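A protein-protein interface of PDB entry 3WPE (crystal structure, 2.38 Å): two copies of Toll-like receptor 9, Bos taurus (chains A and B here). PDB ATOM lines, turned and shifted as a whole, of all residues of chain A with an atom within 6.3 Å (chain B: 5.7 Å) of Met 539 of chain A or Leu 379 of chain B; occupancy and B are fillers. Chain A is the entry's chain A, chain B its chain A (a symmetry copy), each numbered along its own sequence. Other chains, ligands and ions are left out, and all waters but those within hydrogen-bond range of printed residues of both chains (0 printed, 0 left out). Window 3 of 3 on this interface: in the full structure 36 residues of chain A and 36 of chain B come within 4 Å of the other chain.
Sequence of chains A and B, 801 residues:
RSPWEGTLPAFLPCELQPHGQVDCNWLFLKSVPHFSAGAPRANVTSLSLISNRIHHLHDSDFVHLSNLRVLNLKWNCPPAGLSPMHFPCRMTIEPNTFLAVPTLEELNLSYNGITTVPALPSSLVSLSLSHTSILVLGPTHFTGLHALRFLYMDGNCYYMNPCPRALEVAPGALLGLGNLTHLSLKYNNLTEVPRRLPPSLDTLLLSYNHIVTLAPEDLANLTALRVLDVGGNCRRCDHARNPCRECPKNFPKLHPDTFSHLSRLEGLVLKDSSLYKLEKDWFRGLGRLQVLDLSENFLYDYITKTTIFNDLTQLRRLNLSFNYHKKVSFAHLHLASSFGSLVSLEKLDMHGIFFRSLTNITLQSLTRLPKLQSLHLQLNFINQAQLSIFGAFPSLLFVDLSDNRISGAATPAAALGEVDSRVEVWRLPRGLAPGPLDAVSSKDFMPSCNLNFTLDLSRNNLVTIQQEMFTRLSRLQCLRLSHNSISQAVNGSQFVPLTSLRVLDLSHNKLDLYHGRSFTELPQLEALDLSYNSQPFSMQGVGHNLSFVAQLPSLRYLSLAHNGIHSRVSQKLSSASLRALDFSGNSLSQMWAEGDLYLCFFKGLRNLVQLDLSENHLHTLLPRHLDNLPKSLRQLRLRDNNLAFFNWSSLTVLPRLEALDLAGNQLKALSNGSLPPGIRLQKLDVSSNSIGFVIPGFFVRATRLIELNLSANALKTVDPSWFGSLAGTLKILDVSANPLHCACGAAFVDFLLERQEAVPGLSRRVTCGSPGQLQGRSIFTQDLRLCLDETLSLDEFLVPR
The backbone NH (N) of Phe 381 of chain B lies close to the side-chain amide nitrogen (ND2) of Asn 404 of chain B (3.2 Å).
N of Gly 352 of chain B sits close to O of Leu 379 of chain B (3.3 Å).
O of His 351 of chain B lies within hydrogen-bond range of N of Phe 322 of chain B, at 2.8 Å.
N of Leu 379 of chain B lies within hydrogen-bond range of O of Ser 402 of chain B, at 3.3 Å.
N of Leu 379 of chain B is in hydrogen-bond range of O of Asp 403 of chain B, at 3.3 Å.
The side-chain amide oxygen of Gln 540 of chain A lies within hydrogen-bond range of a ring nitrogen (NE2) of His 566 of chain A, 3.0 Å away.
Of the 14 printed residues of chain A, 3 touch a printed residue of chain B.
Hydrophobic or aromatic side chains of chain A within 4 Å of the printed part of chain B: Met 539.
Among the printed residues, 6 pairs touch across the chains.
Among the printed residues, no Asp or Glu carboxylate lies within 4 Å of a Lys or Arg side-chain nitrogen of the other chain.
Leu 379 of chain B touches Met 539 of chain A (CD2 to CE, 3.4 Å).
Met 539 of chain A touches Phe 381 of chain B.
Met 539 of chain A touches Asp 403 of chain B.
Phe 322 of chain B touches Gln 540 of chain A (CZ to O, 3.8 Å).
Leu 379 of chain B touches Gln 540 of chain A.
O of Gly 541 of chain A touches CE1 of Phe 322 of chain B, 3.3 Å away.
Met 539 of chain A touches just these residues of chain B: Leu 379, Phe 381 and Asp 403.
Of the printed residues of chain B, Gln 540 of chain A touches Phe 322 and Leu 379.
Printed residues of chain A within 4 Å of Phe 381 of chain B: Met 539.
The nearest printed residue of chain B that does not touch Met 539 of chain A is Asn 404 of chain B (5.7 Å).
The nearest printed residue of chain B that does not touch Gln 540 of chain A is Asp 403 of chain B (5.8 Å).
No position is printed for both chains.
Of the 6 pairs that touch across the chains among the printed residues, none has its exchanged pair printed and touching as well.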
ATOM      1  N   ASP A 512      27.991  16.640 -27.324  1.00  0.00           N
ATOM      2  CA  ASP A 512      27.956  15.753 -26.171  1.00  0.00           C
ATOM      3  C   ASP A 512      28.838  16.306 -25.056  1.00  0.00           C
ATOM      4  O   ASP A 512      30.061  16.447 -25.210  1.00  0.00           O
ATOM      5  CB  ASP A 512      28.359  14.323 -26.535  1.00  0.00           C
ATOM      6  CG  ASP A 512      27.682  13.301 -25.645  1.00  0.00           C
ATOM      7  OD1 ASP A 512      27.345  13.652 -24.490  1.00  0.00           O
ATOM      8  OD2 ASP A 512      27.471  12.160 -26.101  1.00  0.00           O
ATOM      9  N   SER A 534      19.399  18.822 -27.728  1.00  0.00           N
ATOM     10  CA  SER A 534      18.618  17.852 -26.959  1.00  0.00           C
ATOM     11  C   SER A 534      18.894  16.390 -27.288  1.00  0.00           C
ATOM     12  O   SER A 534      18.564  15.515 -26.499  1.00  0.00           O
ATOM     13  CB  SER A 534      17.128  18.124 -27.161  1.00  0.00           C
ATOM     14  OG  SER A 534      16.834  18.172 -28.538  1.00  0.00           O
ATOM     15  N   GLN A 535      19.491  16.121 -28.439  1.00  0.00           N
ATOM     16  CA  GLN A 535      19.735  14.747 -28.857  1.00  0.00           C
ATOM     17  C   GLN A 535      20.684  14.027 -27.877  1.00  0.00           C
ATOM     18  O   GLN A 535      20.358  12.936 -27.421  1.00  0.00           O
ATOM     19  CB  GLN A 535      20.213  14.697 -30.319  1.00  0.00           C
ATOM     20  CG  GLN A 535      20.460  13.301 -30.884  1.00  0.00           C
ATOM     21  CD  GLN A 535      20.776  13.307 -32.388  1.00  0.00           C
ATOM     22  OE1 GLN A 535      20.233  14.111 -33.155  1.00  0.00           O
ATOM     23  NE2 GLN A 535      21.658  12.408 -32.811  1.00  0.00           N
ATOM     24  N   PRO A 536      21.845  14.631 -27.537  1.00  0.00           N
ATOM     25  CA  PRO A 536      22.669  14.046 -26.455  1.00  0.00           C
ATOM     26  C   PRO A 536      21.968  13.975 -25.100  1.00  0.00           C
ATOM     27  O   PRO A 536      21.956  12.923 -24.481  1.00  0.00           O
ATOM     28  CB  PRO A 536      23.876  14.985 -26.374  1.00  0.00           C
ATOM     29  CG  PRO A 536      23.961  15.607 -27.722  1.00  0.00           C
ATOM     30  CD  PRO A 536      22.571  15.682 -28.267  1.00  0.00           C
ATOM     31  N   PHE A 537      21.379  15.082 -24.660  1.00  0.00           N
ATOM     32  CA  PHE A 537      20.739  15.168 -23.333  1.00  0.00           C
ATOM     33  C   PHE A 537      19.511  14.277 -23.150  1.00  0.00           C
ATOM     34  O   PHE A 537      19.215  13.856 -22.030  1.00  0.00           O
ATOM     35  CB  PHE A 537      20.332  16.611 -23.032  1.00  0.00           C
ATOM     36  CG  PHE A 537      21.477  17.495 -22.652  1.00  0.00           C
ATOM     37  CD1 PHE A 537      22.123  17.319 -21.447  1.00  0.00           C
ATOM     38  CD2 PHE A 537      21.892  18.515 -23.487  1.00  0.00           C
ATOM     39  CE1 PHE A 537      23.170  18.140 -21.080  1.00  0.00           C
ATOM     40  CE2 PHE A 537      22.940  19.342 -23.126  1.00  0.00           C
ATOM     41  CZ  PHE A 537      23.576  19.156 -21.920  1.00  0.00           C
ATOM     42  N   SER A 538      18.792  14.010 -24.238  1.00  0.00           N
ATOM     43  CA  SER A 538      17.603  13.162 -24.184  1.00  0.00           C
ATOM     44  C   SER A 538      17.922  11.673 -24.292  1.00  0.00           C
ATOM     45  O   SER A 538      17.008  10.849 -24.245  1.00  0.00           O
ATOM     46  CB  SER A 538      16.624  13.547 -25.293  1.00  0.00           C
ATOM     47  OG  SER A 538      16.298  14.921 -25.215  1.00  0.00           O
ATOM     48  N   MET A 539      19.200  11.321 -24.455  1.00  0.00           N
ATOM     49  CA  MET A 539      19.606   9.917 -24.413  1.00  0.00           C
ATOM     50  C   MET A 539      19.239   9.353 -23.041  1.00  0.00           C
ATOM     51  O   MET A 539      19.622   9.913 -22.008  1.00  0.00           O
ATOM     52  CB  MET A 539      21.112   9.744 -24.649  1.00  0.00           C
ATOM     53  CG  MET A 539      21.582   9.976 -26.076  1.00  0.00           C
ATOM     54  SD  MET A 539      23.382   9.866 -26.235  1.00  0.00           S
ATOM     55  CE  MET A 539      23.613   8.102 -26.427  1.00  0.00           C
ATOM     56  N   GLN A 540      18.487   8.256 -23.048  1.00  0.00           N
ATOM     57  CA  GLN A 540      18.071   7.589 -21.825  1.00  0.00           C
ATOM     58  C   GLN A 540      19.206   6.702 -21.332  1.00  0.00           C
ATOM     59  O   GLN A 540      19.915   6.093 -22.132  1.00  0.00           O
ATOM     60  CB  GLN A 540      16.822   6.742 -22.079  1.00  0.00           C
ATOM     61  CG  GLN A 540      16.007   6.449 -20.830  1.00  0.00           C
ATOM     62  CD  GLN A 540      15.200   7.649 -20.371  1.00  0.00           C
ATOM     63  OE1 GLN A 540      15.520   8.279 -19.360  1.00  0.00           O
ATOM     64  NE2 GLN A 540      14.149   7.974 -21.116  1.00  0.00           N
ATOM     65  N   GLY A 541      19.380   6.644 -20.014  1.00  0.00           N
ATOM     66  CA  GLY A 541      20.408   5.804 -19.397  1.00  0.00           C
ATOM     67  C   GLY A 541      21.836   6.298 -19.545  1.00  0.00           C
ATOM     68  O   GLY A 541      22.770   5.597 -19.172  1.00  0.00           O
ATOM     69  N   VAL A 542      22.006   7.505 -20.079  1.00  0.00           N
ATOM     70  CA  VAL A 542      23.324   8.103 -20.277  1.00  0.00           C
ATOM     71  C   VAL A 542      23.435   9.342 -19.384  1.00  0.00           C
ATOM     72  O   VAL A 542      22.502  10.139 -19.299  1.00  0.00           O
ATOM     73  CB  VAL A 542      23.535   8.493 -21.757  1.00  0.00           C
ATOM     74  CG1 VAL A 542      24.915   9.094 -21.981  1.00  0.00           C
ATOM     75  CG2 VAL A 542      23.351   7.278 -22.652  1.00  0.00           C
ATOM     76  N   GLY A 543      24.577   9.496 -18.720  1.00  0.00           N
ATOM     77  CA  GLY A 543      24.799  10.621 -17.825  1.00  0.00           C
ATOM     78  C   GLY A 543      25.200  11.889 -18.548  1.00  0.00           C
ATOM     79  O   GLY A 543      25.629  11.848 -19.695  1.00  0.00           O
ATOM     80  N   HIS A 544      25.065  13.023 -17.865  1.00  0.00           N
ATOM     81  CA  HIS A 544      25.461  14.311 -18.425  1.00  0.00           C
ATOM     82  C   HIS A 544      26.079  15.235 -17.367  1.00  0.00           C
ATOM     83  O   HIS A 544      25.419  15.623 -16.405  1.00  0.00           O
ATOM     84  CB  HIS A 544      24.264  14.964 -19.118  1.00  0.00           C
ATOM     85  CG  HIS A 544      23.846  14.251 -20.368  1.00  0.00           C
ATOM     86  ND1 HIS A 544      24.582  14.309 -21.533  1.00  0.00           N
ATOM     87  CD2 HIS A 544      22.797  13.433 -20.623  1.00  0.00           C
ATOM     88  CE1 HIS A 544      23.997  13.570 -22.458  1.00  0.00           C
ATOM     89  NE2 HIS A 544      22.910  13.028 -21.932  1.00  0.00           N
ATOM     90  N   HIS A 566      16.501  15.886 -18.088  1.00  0.00           N
ATOM     91  CA  HIS A 566      15.478  15.291 -17.215  1.00  0.00           C
ATOM     92  C   HIS A 566      16.001  14.356 -16.117  1.00  0.00           C
ATOM     93  O   HIS A 566      15.359  14.227 -15.073  1.00  0.00           O
ATOM     94  CB  HIS A 566      14.401  14.571 -18.049  1.00  0.00           C
ATOM     95  CG  HIS A 566      14.885  13.338 -18.743  1.00  0.00           C
ATOM     96  ND1 HIS A 566      15.423  13.363 -20.013  1.00  0.00           N
ATOM     97  CD2 HIS A 566      14.906  12.045 -18.350  1.00  0.00           C
ATOM     98  CE1 HIS A 566      15.758  12.136 -20.369  1.00  0.00           C
ATOM     99  NE2 HIS A 566      15.457  11.318 -19.377  1.00  0.00           N
ATOM    100  N   SER A 567      17.135  13.692 -16.350  1.00  0.00           N
ATOM    101  CA  SER A 567      17.742  12.835 -15.326  1.00  0.00           C
ATOM    102  C   SER A 567      19.225  12.533 -15.604  1.00  0.00           C
ATOM    103  O   SER A 567      19.777  12.940 -16.631  1.00  0.00           O
ATOM    104  CB  SER A 567      16.943  11.529 -15.197  1.00  0.00           C
ATOM    105  OG  SER A 567      17.027  10.762 -16.376  1.00  0.00           O
ATOM    106  N   PHE B 322      22.748  -2.256 -20.582  1.00  0.00           N
ATOM    107  CA  PHE B 322      23.572  -1.541 -19.608  1.00  0.00           C
ATOM    108  C   PHE B 322      24.486  -2.435 -18.780  1.00  0.00           C
ATOM    109  O   PHE B 322      24.672  -2.233 -17.583  1.00  0.00           O
ATOM    110  CB  PHE B 322      22.705  -0.609 -18.756  1.00  0.00           C
ATOM    111  CG  PHE B 322      22.165   0.550 -19.539  1.00  0.00           C
ATOM    112  CD1 PHE B 322      22.998   1.594 -19.907  1.00  0.00           C
ATOM    113  CD2 PHE B 322      20.843   0.566 -19.967  1.00  0.00           C
ATOM    114  CE1 PHE B 322      22.516   2.653 -20.659  1.00  0.00           C
ATOM    115  CE2 PHE B 322      20.355   1.620 -20.715  1.00  0.00           C
ATOM    116  CZ  PHE B 322      21.194   2.661 -21.066  1.00  0.00           C
ATOM    117  N   HIS B 351      21.428  -3.028 -25.553  1.00  0.00           N
ATOM    118  CA  HIS B 351      21.676  -1.588 -25.625  1.00  0.00           C
ATOM    119  C   HIS B 351      22.417  -1.133 -24.377  1.00  0.00           C
ATOM    120  O   HIS B 351      22.290  -1.743 -23.325  1.00  0.00           O
ATOM    121  CB  HIS B 351      20.380  -0.783 -25.884  1.00  0.00           C
ATOM    122  CG  HIS B 351      19.438  -0.709 -24.722  1.00  0.00           C
ATOM    123  ND1 HIS B 351      18.545  -1.710 -24.425  1.00  0.00           N
ATOM    124  CD2 HIS B 351      19.221   0.269 -23.811  1.00  0.00           C
ATOM    125  CE1 HIS B 351      17.828  -1.365 -23.372  1.00  0.00           C
ATOM    126  NE2 HIS B 351      18.220  -0.169 -22.979  1.00  0.00           N
ATOM    127  N   GLY B 352      23.224  -0.089 -24.517  1.00  0.00           N
ATOM    128  CA  GLY B 352      23.951   0.495 -23.390  1.00  0.00           C
ATOM    129  C   GLY B 352      25.124  -0.302 -22.839  1.00  0.00           C
ATOM    130  O   GLY B 352      25.473  -0.151 -21.673  1.00  0.00           O
ATOM    131  N   ILE B 353      25.717  -1.172 -23.650  1.00  0.00           N
ATOM    132  CA  ILE B 353      26.973  -1.857 -23.279  1.00  0.00           C
ATOM    133  C   ILE B 353      28.210  -1.032 -23.639  1.00  0.00           C
ATOM    134  O   ILE B 353      29.247  -1.147 -22.987  1.00  0.00           O
ATOM    135  CB  ILE B 353      27.070  -3.251 -23.932  1.00  0.00           C
ATOM    136  CG1 ILE B 353      25.983  -4.169 -23.372  1.00  0.00           C
ATOM    137  CG2 ILE B 353      28.443  -3.875 -23.694  1.00  0.00           C
ATOM    138  CD1 ILE B 353      25.715  -5.391 -24.224  1.00  0.00           C
ATOM    139  N   PHE B 354      28.084  -0.208 -24.674  1.00  0.00           N
ATOM    140  CA  PHE B 354      29.138   0.692 -25.158  1.00  0.00           C
ATOM    141  C   PHE B 354      30.271  -0.041 -25.867  1.00  0.00           C
ATOM    142  O   PHE B 354      31.222  -0.503 -25.239  1.00  0.00           O
ATOM    143  CB  PHE B 354      29.698   1.604 -24.052  1.00  0.00           C
ATOM    144  CG  PHE B 354      28.645   2.268 -23.205  1.00  0.00           C
ATOM    145  CD1 PHE B 354      27.432   2.671 -23.747  1.00  0.00           C
ATOM    146  CD2 PHE B 354      28.889   2.520 -21.861  1.00  0.00           C
ATOM    147  CE1 PHE B 354      26.471   3.283 -22.960  1.00  0.00           C
ATOM    148  CE2 PHE B 354      27.933   3.137 -21.066  1.00  0.00           C
ATOM    149  CZ  PHE B 354      26.722   3.521 -21.618  1.00  0.00           C
ATOM    150  N   LEU B 377      20.154  -2.615 -30.261  1.00  0.00           N
ATOM    151  CA  LEU B 377      21.568  -2.241 -30.211  1.00  0.00           C
ATOM    152  C   LEU B 377      21.776  -0.740 -30.053  1.00  0.00           C
ATOM    153  O   LEU B 377      22.854  -0.220 -30.364  1.00  0.00           O
ATOM    154  CB  LEU B 377      22.263  -2.714 -31.493  1.00  0.00           C
ATOM    155  CG  LEU B 377      22.375  -4.232 -31.654  1.00  0.00           C
ATOM    156  CD1 LEU B 377      22.608  -4.612 -33.101  1.00  0.00           C
ATOM    157  CD2 LEU B 377      23.494  -4.775 -30.779  1.00  0.00           C
ATOM    158  N   GLN B 378      20.757  -0.040 -29.561  1.00  0.00           N
ATOM    159  CA  GLN B 378      20.827   1.412 -29.429  1.00  0.00           C
ATOM    160  C   GLN B 378      21.747   1.799 -28.272  1.00  0.00           C
ATOM    161  O   GLN B 378      22.162   0.944 -27.490  1.00  0.00           O
ATOM    162  CB  GLN B 378      19.430   2.043 -29.252  1.00  0.00           C
ATOM    163  CG  GLN B 378      18.673   1.715 -27.968  1.00  0.00           C
ATOM    164  CD  GLN B 378      17.973   0.370 -28.009  1.00  0.00           C
ATOM    165  OE1 GLN B 378      18.204  -0.442 -28.903  1.00  0.00           O
ATOM    166  NE2 GLN B 378      17.116   0.126 -27.036  1.00  0.00           N
ATOM    167  N   LEU B 379      22.085   3.085 -28.202  1.00  0.00           N
ATOM    168  CA  LEU B 379      22.860   3.642 -27.087  1.00  0.00           C
ATOM    169  C   LEU B 379      24.164   2.891 -26.808  1.00  0.00           C
ATOM    170  O   LEU B 379      24.531   2.709 -25.663  1.00  0.00           O
ATOM    171  CB  LEU B 379      21.994   3.691 -25.814  1.00  0.00           C
ATOM    172  CG  LEU B 379      20.690   4.496 -25.928  1.00  0.00           C
ATOM    173  CD1 LEU B 379      19.719   4.182 -24.800  1.00  0.00           C
ATOM    174  CD2 LEU B 379      20.972   5.986 -25.967  1.00  0.00           C
ATOM    175  N   ASN B 380      24.860   2.465 -27.860  1.00  0.00           N
ATOM    176  CA  ASN B 380      26.135   1.751 -27.709  1.00  0.00           C
ATOM    177  C   ASN B 380      27.374   2.581 -28.077  1.00  0.00           C
ATOM    178  O   ASN B 380      28.495   2.098 -27.947  1.00  0.00           O
ATOM    179  CB  ASN B 380      26.132   0.443 -28.532  1.00  0.00           C
ATOM    180  CG  ASN B 380      25.279  -0.658 -27.917  1.00  0.00           C
ATOM    181  OD1 ASN B 380      24.523  -1.329 -28.608  1.00  0.00           O
ATOM    182  ND2 ASN B 380      25.427  -0.877 -26.635  1.00  0.00           N
ATOM    183  N   PHE B 381      27.176   3.823 -28.517  1.00  0.00           N
ATOM    184  CA  PHE B 381      28.266   4.685 -29.014  1.00  0.00           C
ATOM    185  C   PHE B 381      29.069   4.093 -30.179  1.00  0.00           C
ATOM    186  O   PHE B 381      30.267   4.354 -30.311  1.00  0.00           O
ATOM    187  CB  PHE B 381      29.211   5.087 -27.873  1.00  0.00           C
ATOM    188  CG  PHE B 381      28.557   5.927 -26.810  1.00  0.00           C
ATOM    189  CD1 PHE B 381      28.175   7.232 -27.076  1.00  0.00           C
ATOM    190  CD2 PHE B 381      28.328   5.415 -25.538  1.00  0.00           C
ATOM    191  CE1 PHE B 381      27.577   8.013 -26.093  1.00  0.00           C
ATOM    192  CE2 PHE B 381      27.732   6.190 -24.555  1.00  0.00           C
ATOM    193  CZ  PHE B 381      27.354   7.491 -24.832  1.00  0.00           C
ATOM    194  N   SER B 402      19.573   2.959 -33.176  1.00  0.00           N
ATOM    195  CA  SER B 402      19.359   4.380 -32.943  1.00  0.00           C
ATOM    196  C   SER B 402      20.264   4.872 -31.817  1.00  0.00           C
ATOM    197  O   SER B 402      20.908   4.076 -31.144  1.00  0.00           O
ATOM    198  CB  SER B 402      17.894   4.661 -32.604  1.00  0.00           C
ATOM    199  OG  SER B 402      17.585   4.211 -31.295  1.00  0.00           O
ATOM    200  N   ASP B 403      20.325   6.190 -31.641  1.00  0.00           N
ATOM    201  CA  ASP B 403      21.154   6.821 -30.608  1.00  0.00           C
ATOM    202  C   ASP B 403      22.568   6.263 -30.540  1.00  0.00           C
ATOM    203  O   ASP B 403      23.086   5.967 -29.460  1.00  0.00           O
ATOM    204  CB  ASP B 403      20.477   6.720 -29.242  1.00  0.00           C
ATOM    205  CG  ASP B 403      19.444   7.798 -29.029  1.00  0.00           C
ATOM    206  OD1 ASP B 403      19.823   8.988 -29.094  1.00  0.00           O
ATOM    207  OD2 ASP B 403      18.264   7.458 -28.793  1.00  0.00           O
ATOM    208  N   ASN B 404      23.186   6.120 -31.705  1.00  0.00           N
ATOM    209  CA  ASN B 404      24.571   5.698 -31.783  1.00  0.00           C
ATOM    210  C   ASN B 404      25.363   6.848 -32.381  1.00  0.00           C
ATOM    211  O   ASN B 404      24.861   7.973 -32.432  1.00  0.00           O
ATOM    212  CB  ASN B 404      24.679   4.403 -32.594  1.00  0.00           C
ATOM    213  CG  ASN B 404      24.360   3.170 -31.769  1.00  0.00           C
ATOM    214  OD1 ASN B 404      23.340   2.508 -31.961  1.00  0.00           O
ATOM    215  ND2 ASN B 404      25.232   2.860 -30.847  1.00  0.00           N
